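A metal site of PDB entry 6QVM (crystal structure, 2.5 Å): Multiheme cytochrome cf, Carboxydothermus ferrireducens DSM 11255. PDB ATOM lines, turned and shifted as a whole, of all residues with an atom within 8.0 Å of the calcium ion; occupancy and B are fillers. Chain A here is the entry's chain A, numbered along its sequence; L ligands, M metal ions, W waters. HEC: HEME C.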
ATOM      1  N   SER A 380       4.150  15.270 -18.000  1.00  0.00           N
ATOM      2  CA  SER A 380       4.501  15.386 -19.409  1.00  0.00           C
ATOM      3  C   SER A 380       5.309  14.196 -19.900  1.00  0.00           C
ATOM      4  O   SER A 380       5.343  13.948 -21.110  1.00  0.00           O
ATOM      5  CB  SER A 380       5.294  16.663 -19.650  1.00  0.00           C
ATOM      6  OG  SER A 380       4.506  17.803 -19.348  1.00  0.00           O
ATOM      7  N   ALA A 381       5.952  13.461 -18.992  1.00  0.00           N
ATOM      8  CA  ALA A 381       6.749  12.305 -19.404  1.00  0.00           C
ATOM      9  C   ALA A 381       5.902  11.241 -20.076  1.00  0.00           C
ATOM     10  O   ALA A 381       6.416  10.436 -20.861  1.00  0.00           O
ATOM     11  CB  ALA A 381       7.490  11.723 -18.204  1.00  0.00           C
ATOM     12  N   GLU A 384       6.200  12.659 -23.546  1.00  0.00           N
ATOM     13  CA  GLU A 384       7.514  13.002 -24.064  1.00  0.00           C
ATOM     14  C   GLU A 384       8.285  11.799 -24.587  1.00  0.00           C
ATOM     15  O   GLU A 384       9.255  11.986 -25.325  1.00  0.00           O
ATOM     16  CB  GLU A 384       8.334  13.708 -22.984  1.00  0.00           C
ATOM     17  CG  GLU A 384       7.989  15.177 -22.810  1.00  0.00           C
ATOM     18  CD  GLU A 384       8.552  15.765 -21.523  1.00  0.00           C
ATOM     19  OE1 GLU A 384       8.600  15.035 -20.516  1.00  0.00           O
ATOM     20  OE2 GLU A 384       8.965  16.941 -21.529  1.00  0.00           O
ATOM     21  N   HIS A 387       6.810  12.361 -28.080  1.00  0.00           N
ATOM     22  CA  HIS A 387       6.988  13.770 -28.421  1.00  0.00           C
ATOM     23  C   HIS A 387       8.215  14.307 -27.681  1.00  0.00           C
ATOM     24  O   HIS A 387       8.108  15.109 -26.748  1.00  0.00           O
ATOM     25  CB  HIS A 387       5.749  14.574 -28.072  1.00  0.00           C
ATOM     26  CG  HIS A 387       4.476  14.064 -28.690  1.00  0.00           C
ATOM     27  ND1 HIS A 387       3.899  14.669 -29.783  1.00  0.00           N
ATOM     28  CD2 HIS A 387       3.653  13.056 -28.330  1.00  0.00           C
ATOM     29  CE1 HIS A 387       2.783  14.023 -30.104  1.00  0.00           C
ATOM     30  NE2 HIS A 387       2.612  13.048 -29.229  1.00  0.00           N
ATOM     31  N   GLU A 388       9.391  13.860 -28.116  1.00  0.00           N
ATOM     32  CA  GLU A 388      10.576  14.058 -27.306  1.00  0.00           C
ATOM     33  C   GLU A 388      11.082  15.488 -27.297  1.00  0.00           C
ATOM     34  O   GLU A 388      11.886  15.850 -26.432  1.00  0.00           O
ATOM     35  CB  GLU A 388      11.702  13.131 -27.779  1.00  0.00           C
ATOM     36  CG  GLU A 388      12.516  13.647 -28.949  1.00  0.00           C
ATOM     37  CD  GLU A 388      11.758  13.633 -30.262  1.00  0.00           C
ATOM     38  OE1 GLU A 388      11.739  14.675 -30.951  1.00  0.00           O
ATOM     39  OE2 GLU A 388      11.211  12.575 -30.621  1.00  0.00           O
ATOM     40  N   GLY A 389      10.636  16.322 -28.237  1.00  0.00           N
ATOM     41  CA  GLY A 389      11.032  17.722 -28.271  1.00  0.00           C
ATOM     42  C   GLY A 389      12.146  18.060 -29.245  1.00  0.00           C
ATOM     43  O   GLY A 389      12.544  19.229 -29.306  1.00  0.00           O
ATOM     44  N   GLY A 394       6.429  19.457 -28.720  1.00  0.00           N
ATOM     45  CA  GLY A 394       5.818  19.394 -27.405  1.00  0.00           C
ATOM     46  C   GLY A 394       6.826  19.320 -26.273  1.00  0.00           C
ATOM     47  O   GLY A 394       6.758  20.107 -25.332  1.00  0.00           O
ATOM     48  N   GLY A 395       7.776  18.379 -26.367  1.00  0.00           N
ATOM     49  CA  GLY A 395       8.686  18.130 -25.266  1.00  0.00           C
ATOM     50  C   GLY A 395       9.546  19.322 -24.872  1.00  0.00           C
ATOM     51  O   GLY A 395       9.935  19.443 -23.703  1.00  0.00           O
ATOM     52  N   GLU A 396       9.833  20.217 -25.821  1.00  0.00           N
ATOM     53  CA  GLU A 396      10.740  21.326 -25.546  1.00  0.00           C
ATOM     54  C   GLU A 396      10.164  22.330 -24.541  1.00  0.00           C
ATOM     55  O   GLU A 396      10.921  23.151 -24.027  1.00  0.00           O
ATOM     56  CB  GLU A 396      11.092  22.063 -26.837  1.00  0.00           C
ATOM     57  CG  GLU A 396       9.905  22.723 -27.524  1.00  0.00           C
ATOM     58  CD  GLU A 396       9.266  21.834 -28.584  1.00  0.00           C
ATOM     59  OE1 GLU A 396       8.769  22.388 -29.596  1.00  0.00           O
ATOM     60  OE2 GLU A 396       9.264  20.597 -28.405  1.00  0.00           O
ATOM     61  N   TYR A 397       8.865  22.266 -24.258  1.00  0.00           N
ATOM     62  CA  TYR A 397       8.221  23.305 -23.456  1.00  0.00           C
ATOM     63  C   TYR A 397       8.796  23.419 -22.047  1.00  0.00           C
ATOM     64  O   TYR A 397       8.671  24.471 -21.425  1.00  0.00           O
ATOM     65  CB  TYR A 397       6.712  23.039 -23.380  1.00  0.00           C
ATOM     66  CG  TYR A 397       6.288  22.291 -22.136  1.00  0.00           C
ATOM     67  CD1 TYR A 397       6.476  20.926 -22.033  1.00  0.00           C
ATOM     68  CD2 TYR A 397       5.702  22.956 -21.067  1.00  0.00           C
ATOM     69  CE1 TYR A 397       6.103  20.232 -20.897  1.00  0.00           C
ATOM     70  CE2 TYR A 397       5.311  22.278 -19.927  1.00  0.00           C
ATOM     71  CZ  TYR A 397       5.518  20.910 -19.848  1.00  0.00           C
ATOM     72  OH  TYR A 397       5.135  20.231 -18.714  1.00  0.00           O
ATOM     73  N   ASN A 398       9.422  22.347 -21.521  1.00  0.00           N
ATOM     74  CA  ASN A 398      10.011  22.373 -20.190  1.00  0.00           C
ATOM     75  C   ASN A 398      11.506  22.100 -20.213  1.00  0.00           C
ATOM     76  O   ASN A 398      12.083  21.700 -19.190  1.00  0.00           O
ATOM     77  CB  ASN A 398       9.306  21.378 -19.261  1.00  0.00           C
ATOM     78  CG  ASN A 398       9.396  19.941 -19.748  1.00  0.00           C
ATOM     79  OD1 ASN A 398      10.060  19.632 -20.732  1.00  0.00           O
ATOM     80  ND2 ASN A 398       8.719  19.039 -19.046  1.00  0.00           N
ATOM     81  N   ASP A 399      12.154  22.294 -21.355  1.00  0.00           N
ATOM     82  CA  ASP A 399      13.562  21.966 -21.506  1.00  0.00           C
ATOM     83  C   ASP A 399      14.435  23.135 -21.066  1.00  0.00           C
ATOM     84  O   ASP A 399      13.959  24.207 -20.680  1.00  0.00           O
ATOM     85  CB  ASP A 399      13.853  21.573 -22.958  1.00  0.00           C
ATOM     86  CG  ASP A 399      13.381  20.175 -23.292  1.00  0.00           C
ATOM     87  OD1 ASP A 399      12.820  19.510 -22.388  1.00  0.00           O
ATOM     88  OD2 ASP A 399      13.577  19.734 -24.450  1.00  0.00           O
ATOM     89  N   GLU A 400      15.752  22.932 -21.141  1.00  0.00           N
ATOM     90  CA  GLU A 400      16.746  23.942 -20.832  1.00  0.00           C
ATOM     91  C   GLU A 400      17.305  24.504 -22.139  1.00  0.00           C
ATOM     92  O   GLU A 400      17.752  23.746 -23.001  1.00  0.00           O
ATOM     93  CB  GLU A 400      17.869  23.342 -19.988  1.00  0.00           C
ATOM     94  CG  GLU A 400      18.983  24.300 -19.611  1.00  0.00           C
ATOM     95  CD  GLU A 400      20.064  23.629 -18.767  1.00  0.00           C
ATOM     96  OE1 GLU A 400      20.844  24.344 -18.112  1.00  0.00           O
ATOM     97  OE2 GLU A 400      20.107  22.373 -18.769  1.00  0.00           O
ATOM     98  N   TYR A 401      17.271  25.833 -22.275  1.00  0.00           N
ATOM     99  CA  TYR A 401      17.604  26.496 -23.532  1.00  0.00           C
ATOM    100  C   TYR A 401      18.886  27.297 -23.398  1.00  0.00           C
ATOM    101  O   TYR A 401      19.103  27.989 -22.405  1.00  0.00           O
ATOM    102  CB  TYR A 401      16.496  27.462 -23.970  1.00  0.00           C
ATOM    103  CG  TYR A 401      15.078  26.982 -23.832  1.00  0.00           C
ATOM    104  CD1 TYR A 401      14.741  25.645 -24.040  1.00  0.00           C
ATOM    105  CD2 TYR A 401      14.063  27.875 -23.509  1.00  0.00           C
ATOM    106  CE1 TYR A 401      13.437  25.214 -23.915  1.00  0.00           C
ATOM    107  CE2 TYR A 401      12.762  27.453 -23.382  1.00  0.00           C
ATOM    108  CZ  TYR A 401      12.452  26.128 -23.591  1.00  0.00           C
ATOM    109  OH  TYR A 401      11.146  25.718 -23.456  1.00  0.00           O
ATOM    110  N   ASN A 572      18.820  23.262 -27.485  1.00  0.00           N
ATOM    111  CA  ASN A 572      18.091  22.555 -26.436  1.00  0.00           C
ATOM    112  C   ASN A 572      19.071  21.650 -25.717  1.00  0.00           C
ATOM    113  O   ASN A 572      19.420  20.574 -26.199  1.00  0.00           O
ATOM    114  CB  ASN A 572      16.924  21.782 -27.043  1.00  0.00           C
ATOM    115  CG  ASN A 572      15.925  21.331 -26.007  1.00  0.00           C
ATOM    116  OD1 ASN A 572      16.293  20.964 -24.885  1.00  0.00           O
ATOM    117  ND2 ASN A 572      14.645  21.357 -26.361  1.00  0.00           N
ATOM    118  N   THR A 574      18.592  20.046 -22.940  1.00  0.00           N
ATOM    119  CA  THR A 574      17.945  18.830 -22.469  1.00  0.00           C
ATOM    120  C   THR A 574      18.011  17.731 -23.524  1.00  0.00           C
ATOM    121  O   THR A 574      18.303  16.573 -23.210  1.00  0.00           O
ATOM    122  CB  THR A 574      16.497  19.100 -22.084  1.00  0.00           C
ATOM    123  OG1 THR A 574      16.428  20.226 -21.188  1.00  0.00           O
ATOM    124  CG2 THR A 574      15.897  17.885 -21.397  1.00  0.00           C
ATOM    125  N   ILE A 575      17.768  18.089 -24.785  1.00  0.00           N
ATOM    126  CA  ILE A 575      17.927  17.136 -25.878  1.00  0.00           C
ATOM    127  C   ILE A 575      19.393  16.743 -26.014  1.00  0.00           C
ATOM    128  O   ILE A 575      19.730  15.551 -26.166  1.00  0.00           O
ATOM    129  CB  ILE A 575      17.396  17.741 -27.194  1.00  0.00           C
ATOM    130  CG1 ILE A 575      15.926  18.145 -27.051  1.00  0.00           C
ATOM    131  CG2 ILE A 575      17.584  16.767 -28.348  1.00  0.00           C
ATOM    132  CD1 ILE A 575      15.037  17.015 -26.601  1.00  0.00           C
ATOM    133  N   ASP A 578      21.046  13.924 -23.473  1.00  0.00           N
ATOM    134  CA  ASP A 578      20.176  12.789 -23.158  1.00  0.00           C
ATOM    135  C   ASP A 578      20.464  11.671 -24.169  1.00  0.00           C
ATOM    136  O   ASP A 578      19.969  11.718 -25.297  1.00  0.00           O
ATOM    137  CB  ASP A 578      18.709  13.197 -23.174  1.00  0.00           C
ATOM    138  CG  ASP A 578      17.790  12.086 -22.649  1.00  0.00           C
ATOM    139  OD1 ASP A 578      18.271  10.953 -22.426  1.00  0.00           O
ATOM    140  OD2 ASP A 578      16.586  12.361 -22.469  1.00  0.00           O
HETATM  141 FE   HEC L   1       1.193  21.445 -27.394  1.00  0.00          FE
HETATM  142  CHA HEC L   1       0.656  22.211 -30.696  1.00  0.00           C
HETATM  143  CHB HEC L   1       2.053  18.259 -28.277  1.00  0.00           C
HETATM  144  CHC HEC L   1       2.167  20.835 -24.135  1.00  0.00           C
HETATM  145  CHD HEC L   1      -0.429  24.288 -26.358  1.00  0.00           C
HETATM  146  NA  HEC L   1       1.303  20.405 -29.149  1.00  0.00           N
HETATM  147  C1A HEC L   1       1.056  20.915 -30.412  1.00  0.00           C
HETATM  148  C2A HEC L   1       1.323  19.870 -31.371  1.00  0.00           C
HETATM  149  C3A HEC L   1       1.709  18.771 -30.701  1.00  0.00           C
HETATM  150  C4A HEC L   1       1.702  19.095 -29.296  1.00  0.00           C
HETATM  151  CMA HEC L   1       2.078  17.423 -31.333  1.00  0.00           C
HETATM  152  CAA HEC L   1       1.199  20.008 -32.906  1.00  0.00           C
HETATM  153  CBA HEC L   1       2.459  20.776 -33.357  1.00  0.00           C
HETATM  154  CGA HEC L   1       2.410  21.060 -34.832  1.00  0.00           C
HETATM  155  O1A HEC L   1       3.231  20.451 -35.556  1.00  0.00           O
HETATM  156  O2A HEC L   1       1.567  21.893 -35.269  1.00  0.00           O
HETATM  157  NB  HEC L   1       1.941  19.855 -26.388  1.00  0.00           N
HETATM  158  C1B HEC L   1       2.309  18.650 -26.979  1.00  0.00           C
HETATM  159  C2B HEC L   1       3.031  17.884 -25.982  1.00  0.00           C
HETATM  160  C3B HEC L   1       3.045  18.575 -24.832  1.00  0.00           C
HETATM  161  C4B HEC L   1       2.372  19.841 -25.075  1.00  0.00           C
HETATM  162  CMB HEC L   1       3.596  16.470 -26.230  1.00  0.00           C
HETATM  163  CAB HEC L   1       3.706  18.167 -23.484  1.00  0.00           C
HETATM  164  CBB HEC L   1       5.234  17.923 -23.614  1.00  0.00           C
HETATM  165  NC  HEC L   1       0.847  22.341 -25.577  1.00  0.00           N
HETATM  166  C1C HEC L   1       1.440  21.981 -24.379  1.00  0.00           C
HETATM  167  C2C HEC L   1       1.157  23.003 -23.382  1.00  0.00           C
HETATM  168  C3C HEC L   1       0.507  24.015 -24.013  1.00  0.00           C
HETATM  169  C4C HEC L   1       0.264  23.578 -25.385  1.00  0.00           C
HETATM  170  CMC HEC L   1       1.715  22.988 -21.937  1.00  0.00           C
HETATM  171  CAC HEC L   1      -0.038  25.340 -23.396  1.00  0.00           C
HETATM  172  CBC HEC L   1       1.066  26.213 -22.751  1.00  0.00           C
HETATM  173  ND  HEC L   1       0.257  22.999 -28.376  1.00  0.00           N
HETATM  174  C1D HEC L   1      -0.342  24.078 -27.719  1.00  0.00           C
HETATM  175  C2D HEC L   1      -0.882  24.955 -28.722  1.00  0.00           C
HETATM  176  C3D HEC L   1      -0.551  24.317 -30.069  1.00  0.00           C
HETATM  177  C4D HEC L   1       0.178  23.108 -29.764  1.00  0.00           C
HETATM  178  CMD HEC L   1      -1.643  26.276 -28.478  1.00  0.00           C
HETATM  179  CAD HEC L   1      -0.897  24.882 -31.460  1.00  0.00           C
HETATM  180  CBD HEC L   1       0.397  25.474 -32.020  1.00  0.00           C
HETATM  181  CGD HEC L   1       0.140  26.215 -33.302  1.00  0.00           C
HETATM  182  O1D HEC L   1       1.053  26.219 -34.171  1.00  0.00           O
HETATM  183  O2D HEC L   1      -0.981  26.786 -33.463  1.00  0.00           O
HETATM  184 CA    CA M   1      11.049  17.925 -22.144  1.00  0.00          CA
HETATM  185  O   HOH W   1      11.686  15.499 -22.125  1.00  0.00           O
HETATM  186  O   HOH W   2      12.299  17.356 -19.887  1.00  0.00           O
HETATM  187  O   HOH W   3      12.144  17.431 -24.317  1.00  0.00           O
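The backbone NH (N) of Ala 381 sits at hydrogen-bond distance from the side-chain carboxylate (OE1) of Glu 384 (3.4 Å). OD2 of Asp 399 lies within hydrogen-bond range of ND2 of Asn 572 (2.7 Å). The backbone NH (N) of Gly 395 lies within hydrogen-bond range of the backbone carbonyl oxygen (O) of His 387 (3.3 Å).
Along chain A the residues within 4 Å of the calcium ion span positions 384 to 399. The nearest printed residue that does not touch the calcium ion is Glu 396 (4.5 Å).
The calcium ion is bound by OE2 of Glu 384 (2.4 Å), OD1 of Asp 399 (2.4 Å), OD1 of Asn 398 (2.4 Å), O of Gly 395 (2.4 Å), water W3 (2.5 Å), water W1 (2.5 Å) and water W2 (2.6 Å).
Water W3 lies within hydrogen-bond range of O of Glu 388 and OD2 of Asp 399.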
